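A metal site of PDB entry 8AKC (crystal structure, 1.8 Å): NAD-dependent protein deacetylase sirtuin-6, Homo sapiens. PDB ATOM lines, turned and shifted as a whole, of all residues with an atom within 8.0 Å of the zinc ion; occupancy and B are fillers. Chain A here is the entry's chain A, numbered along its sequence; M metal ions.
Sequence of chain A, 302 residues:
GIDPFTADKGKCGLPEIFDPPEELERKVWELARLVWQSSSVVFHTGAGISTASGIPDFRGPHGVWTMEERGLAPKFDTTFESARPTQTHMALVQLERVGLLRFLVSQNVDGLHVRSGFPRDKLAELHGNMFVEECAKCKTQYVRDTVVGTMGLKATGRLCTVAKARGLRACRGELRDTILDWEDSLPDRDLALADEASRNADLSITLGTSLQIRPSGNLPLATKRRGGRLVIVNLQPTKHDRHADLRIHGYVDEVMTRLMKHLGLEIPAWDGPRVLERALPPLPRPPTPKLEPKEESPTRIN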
ATOM      1  N   GLU A 134     -30.819  16.369  26.855  1.00  0.00           N
ATOM      2  CA  GLU A 134     -29.509  16.469  26.178  1.00  0.00           C
ATOM      3  C   GLU A 134     -29.484  15.411  25.075  1.00  0.00           C
ATOM      4  O   GLU A 134     -29.895  14.268  25.361  1.00  0.00           O
ATOM      5  CB  GLU A 134     -28.391  16.264  27.198  1.00  0.00           C
ATOM      6  CG  GLU A 134     -27.006  16.258  26.598  1.00  0.00           C
ATOM      7  CD  GLU A 134     -25.908  16.223  27.649  1.00  0.00           C
ATOM      8  OE1 GLU A 134     -25.942  17.086  28.556  1.00  0.00           O
ATOM      9  OE2 GLU A 134     -25.044  15.316  27.561  1.00  0.00           O
ATOM     10  N   CYS A 135     -28.992  15.792  23.894  1.00  0.00           N
ATOM     11  CA  CYS A 135     -28.822  14.878  22.720  1.00  0.00           C
ATOM     12  C   CYS A 135     -27.613  13.977  22.955  1.00  0.00           C
ATOM     13  O   CYS A 135     -26.485  14.506  23.083  1.00  0.00           O
ATOM     14  CB  CYS A 135     -28.664  15.660  21.423  1.00  0.00           C
ATOM     15  SG  CYS A 135     -28.217  14.626  20.014  1.00  0.00           S
ATOM     16  N   ALA A 136     -27.827  12.649  23.019  1.00  0.00           N
ATOM     17  CA  ALA A 136     -26.764  11.618  23.139  1.00  0.00           C
ATOM     18  C   ALA A 136     -25.720  11.800  22.024  1.00  0.00           C
ATOM     19  O   ALA A 136     -24.516  11.646  22.303  1.00  0.00           O
ATOM     20  CB  ALA A 136     -27.377  10.245  23.127  1.00  0.00           C
ATOM     21  N   LYS A 137     -26.143  12.161  20.803  1.00  0.00           N
ATOM     22  CA  LYS A 137     -25.203  12.352  19.662  1.00  0.00           C
ATOM     23  C   LYS A 137     -24.387  13.639  19.829  1.00  0.00           C
ATOM     24  O   LYS A 137     -23.176  13.522  20.090  1.00  0.00           O
ATOM     25  CB  LYS A 137     -25.941  12.359  18.319  1.00  0.00           C
ATOM     26  CG  LYS A 137     -26.509  11.009  17.907  1.00  0.00           C
ATOM     27  CD  LYS A 137     -27.055  10.986  16.498  1.00  0.00           C
ATOM     28  CE  LYS A 137     -27.369   9.583  16.015  1.00  0.00           C
ATOM     29  NZ  LYS A 137     -28.269   9.603  14.847  1.00  0.00           N
ATOM     30  N   CYS A 138     -25.013  14.809  19.684  1.00  0.00           N
ATOM     31  CA  CYS A 138     -24.320  16.117  19.494  1.00  0.00           C
ATOM     32  C   CYS A 138     -24.161  16.869  20.834  1.00  0.00           C
ATOM     33  O   CYS A 138     -23.529  17.949  20.824  1.00  0.00           O
ATOM     34  CB  CYS A 138     -25.034  16.983  18.458  1.00  0.00           C
ATOM     35  SG  CYS A 138     -26.725  17.487  18.890  1.00  0.00           S
ATOM     36  N   LYS A 139     -24.707  16.342  21.935  1.00  0.00           N
ATOM     37  CA  LYS A 139     -24.609  16.914  23.306  1.00  0.00           C
ATOM     38  C   LYS A 139     -25.398  18.229  23.412  1.00  0.00           C
ATOM     39  O   LYS A 139     -25.219  18.950  24.445  1.00  0.00           O
ATOM     40  CB  LYS A 139     -23.138  17.153  23.671  1.00  0.00           C
ATOM     41  CG  LYS A 139     -22.221  15.958  23.453  1.00  0.00           C
ATOM     42  CD  LYS A 139     -22.670  14.719  24.171  1.00  0.00           C
ATOM     43  CE  LYS A 139     -21.652  13.597  24.099  1.00  0.00           C
ATOM     44  NZ  LYS A 139     -22.209  12.327  24.590  1.00  0.00           N
ATOM     45  N   THR A 140     -26.217  18.553  22.415  1.00  0.00           N
ATOM     46  CA  THR A 140     -27.024  19.804  22.414  1.00  0.00           C
ATOM     47  C   THR A 140     -28.045  19.688  23.544  1.00  0.00           C
ATOM     48  O   THR A 140     -28.725  18.654  23.612  1.00  0.00           O
ATOM     49  CB  THR A 140     -27.702  20.088  21.075  1.00  0.00           C
ATOM     50  OG1 THR A 140     -26.678  20.533  20.184  1.00  0.00           O
ATOM     51  CG2 THR A 140     -28.801  21.127  21.175  1.00  0.00           C
ATOM     52  N   GLN A 141     -28.135  20.714  24.386  1.00  0.00           N
ATOM     53  CA  GLN A 141     -29.101  20.759  25.511  1.00  0.00           C
ATOM     54  C   GLN A 141     -30.311  21.607  25.147  1.00  0.00           C
ATOM     55  O   GLN A 141     -30.152  22.621  24.419  1.00  0.00           O
ATOM     56  CB  GLN A 141     -28.403  21.264  26.759  1.00  0.00           C
ATOM     57  CG  GLN A 141     -27.396  20.260  27.261  1.00  0.00           C
ATOM     58  CD  GLN A 141     -26.829  20.691  28.599  1.00  0.00           C
ATOM     59  OE1 GLN A 141     -26.804  21.865  28.899  1.00  0.00           O
ATOM     60  NE2 GLN A 141     -26.391  19.731  29.388  1.00  0.00           N
ATOM     61  N   TYR A 142     -31.474  21.161  25.594  1.00  0.00           N
ATOM     62  CA  TYR A 142     -32.780  21.840  25.403  1.00  0.00           C
ATOM     63  C   TYR A 142     -33.316  22.146  26.803  1.00  0.00           C
ATOM     64  O   TYR A 142     -33.376  21.199  27.628  1.00  0.00           O
ATOM     65  CB  TYR A 142     -33.728  20.946  24.604  1.00  0.00           C
ATOM     66  CG  TYR A 142     -33.230  20.544  23.236  1.00  0.00           C
ATOM     67  CD1 TYR A 142     -32.332  19.505  23.088  1.00  0.00           C
ATOM     68  CD2 TYR A 142     -33.682  21.195  22.096  1.00  0.00           C
ATOM     69  CE1 TYR A 142     -31.882  19.117  21.831  1.00  0.00           C
ATOM     70  CE2 TYR A 142     -33.266  20.794  20.830  1.00  0.00           C
ATOM     71  CZ  TYR A 142     -32.371  19.750  20.703  1.00  0.00           C
ATOM     72  OH  TYR A 142     -31.943  19.345  19.466  1.00  0.00           O
ATOM     73  N   LEU A 159     -36.544  13.743  19.939  1.00  0.00           N
ATOM     74  CA  LEU A 159     -35.328  13.639  19.096  1.00  0.00           C
ATOM     75  C   LEU A 159     -34.736  15.030  18.870  1.00  0.00           C
ATOM     76  O   LEU A 159     -35.471  16.030  18.923  1.00  0.00           O
ATOM     77  CB  LEU A 159     -35.668  12.994  17.753  1.00  0.00           C
ATOM     78  CG  LEU A 159     -36.130  11.528  17.794  1.00  0.00           C
ATOM     79  CD1 LEU A 159     -36.267  10.992  16.381  1.00  0.00           C
ATOM     80  CD2 LEU A 159     -35.153  10.669  18.603  1.00  0.00           C
ATOM     81  N   CYS A 160     -33.439  15.050  18.638  1.00  0.00           N
ATOM     82  CA  CYS A 160     -32.632  16.275  18.389  1.00  0.00           C
ATOM     83  C   CYS A 160     -33.097  16.947  17.101  1.00  0.00           C
ATOM     84  O   CYS A 160     -33.319  16.227  16.102  1.00  0.00           O
ATOM     85  CB  CYS A 160     -31.168  15.903  18.287  1.00  0.00           C
ATOM     86  SG  CYS A 160     -30.092  17.331  18.476  1.00  0.00           S
ATOM     87  N   THR A 161     -33.269  18.263  17.134  1.00  0.00           N
ATOM     88  CA  THR A 161     -33.774  19.088  16.000  1.00  0.00           C
ATOM     89  C   THR A 161     -32.645  19.985  15.449  1.00  0.00           C
ATOM     90  O   THR A 161     -32.963  20.952  14.757  1.00  0.00           O
ATOM     91  CB  THR A 161     -35.012  19.907  16.430  1.00  0.00           C
ATOM     92  OG1 THR A 161     -34.656  20.636  17.603  1.00  0.00           O
ATOM     93  CG2 THR A 161     -36.222  19.050  16.747  1.00  0.00           C
ATOM     94  N   VAL A 162     -31.380  19.665  15.757  1.00  0.00           N
ATOM     95  CA  VAL A 162     -30.210  20.499  15.325  1.00  0.00           C
ATOM     96  C   VAL A 162     -30.111  20.431  13.791  1.00  0.00           C
ATOM     97  O   VAL A 162     -30.121  19.301  13.257  1.00  0.00           O
ATOM     98  CB  VAL A 162     -28.903  20.055  16.007  1.00  0.00           C
ATOM     99  CG1 VAL A 162     -27.666  20.554  15.268  1.00  0.00           C
ATOM    100  CG2 VAL A 162     -28.847  20.492  17.462  1.00  0.00           C
ATOM    101  N   ALA A 163     -30.001  21.604  13.142  1.00  0.00           N
ATOM    102  CA  ALA A 163     -30.071  21.816  11.675  1.00  0.00           C
ATOM    103  C   ALA A 163     -29.346  20.682  10.920  1.00  0.00           C
ATOM    104  O   ALA A 163     -28.097  20.675  10.962  1.00  0.00           O
ATOM    105  CB  ALA A 163     -29.488  23.157  11.325  1.00  0.00           C
ATOM    106  N   CYS A 171     -30.070  15.977  13.071  1.00  0.00           N
ATOM    107  CA  CYS A 171     -29.333  15.055  13.981  1.00  0.00           C
ATOM    108  C   CYS A 171     -30.233  13.886  14.408  1.00  0.00           C
ATOM    109  O   CYS A 171     -29.722  12.749  14.508  1.00  0.00           O
ATOM    110  CB  CYS A 171     -28.837  15.805  15.208  1.00  0.00           C
ATOM    111  SG  CYS A 171     -28.136  14.716  16.469  1.00  0.00           S
ATOM    112  N   ARG A 172     -31.507  14.172  14.691  1.00  0.00           N
ATOM    113  CA  ARG A 172     -32.531  13.188  15.138  1.00  0.00           C
ATOM    114  C   ARG A 172     -31.940  12.306  16.256  1.00  0.00           C
ATOM    115  O   ARG A 172     -32.433  11.186  16.472  1.00  0.00           O
ATOM    116  CB  ARG A 172     -33.083  12.373  13.952  1.00  0.00           C
ATOM    117  CG  ARG A 172     -33.536  13.230  12.774  1.00  0.00           C
ATOM    118  CD  ARG A 172     -34.702  12.695  11.968  1.00  0.00           C
ATOM    119  NE  ARG A 172     -34.879  11.249  12.068  1.00  0.00           N
ATOM    120  CZ  ARG A 172     -35.910  10.641  12.664  1.00  0.00           C
ATOM    121  NH1 ARG A 172     -36.880  11.350  13.209  1.00  0.00           N
ATOM    122  NH2 ARG A 172     -35.948   9.321  12.720  1.00  0.00           N
ATOM    123  N   GLY A 173     -30.927  12.822  16.956  1.00  0.00           N
ATOM    124  CA  GLY A 173     -30.316  12.152  18.126  1.00  0.00           C
ATOM    125  C   GLY A 173     -31.338  11.926  19.226  1.00  0.00           C
ATOM    126  O   GLY A 173     -32.315  12.705  19.315  1.00  0.00           O
ATOM    127  N   GLU A 174     -31.123  10.870  20.004  1.00  0.00           N
ATOM    128  CA  GLU A 174     -31.924  10.515  21.212  1.00  0.00           C
ATOM    129  C   GLU A 174     -31.732  11.592  22.277  1.00  0.00           C
ATOM    130  O   GLU A 174     -30.558  11.842  22.657  1.00  0.00           O
ATOM    131  CB  GLU A 174     -31.472   9.147  21.719  1.00  0.00           C
ATOM    132  CG  GLU A 174     -32.310   8.577  22.842  1.00  0.00           C
ATOM    133  CD  GLU A 174     -32.178   7.074  22.970  1.00  0.00           C
ATOM    134  OE1 GLU A 174     -32.420   6.387  21.946  1.00  0.00           O
ATOM    135  OE2 GLU A 174     -31.810   6.584  24.063  1.00  0.00           O
ATOM    136  N   LEU A 175     -32.816  12.233  22.717  1.00  0.00           N
ATOM    137  CA  LEU A 175     -32.780  13.177  23.874  1.00  0.00           C
ATOM    138  C   LEU A 175     -32.956  12.355  25.145  1.00  0.00           C
ATOM    139  O   LEU A 175     -33.802  11.450  25.148  1.00  0.00           O
ATOM    140  CB  LEU A 175     -33.859  14.253  23.757  1.00  0.00           C
ATOM    141  CG  LEU A 175     -33.777  15.156  22.516  1.00  0.00           C
ATOM    142  CD1 LEU A 175     -34.757  16.318  22.656  1.00  0.00           C
ATOM    143  CD2 LEU A 175     -32.369  15.668  22.276  1.00  0.00           C
HETATM  144 ZN    ZN M   1     -28.310  16.227  18.426  1.00  0.00          ZN
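The backbone NH (N) of Arg 172 lies within hydrogen-bond range of the backbone carbonyl oxygen (O) of Cys 160 (3.1 Å).
The backbone carbonyl oxygen of Cys 171 lies within hydrogen-bond range of the side-chain amino group of Lys 137 (3.5 Å).
The backbone NH of Cys 135 sits at hydrogen-bond distance from the backbone carbonyl oxygen of Thr 140, 2.9 Å away.
O of Val 162 sits at hydrogen-bond distance from N of Cys 171 (3.3 Å).
OH of Tyr 142 lies close to SG of Cys 160, 2.9 Å away.
SG of Cys 135 sits close to N of Lys 137 (3.3 Å).
The side-chain sulfur (SG) of Cys 171 lies close to the backbone NH (N) of Gly 173 (3.4 Å).
The side-chain sulfur (SG) of Cys 138 lies close to the side-chain hydroxyl (OG1) of Thr 140 (3.3 Å).
Of the 19 residues printed, 4 come within 4 Å of the zinc ion.
The zinc ion is bound by SG of Cys 138, SG of Cys 160, SG of Cys 135 and SG of Cys 171.
The zinc ion has four donor atoms within binding distance.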
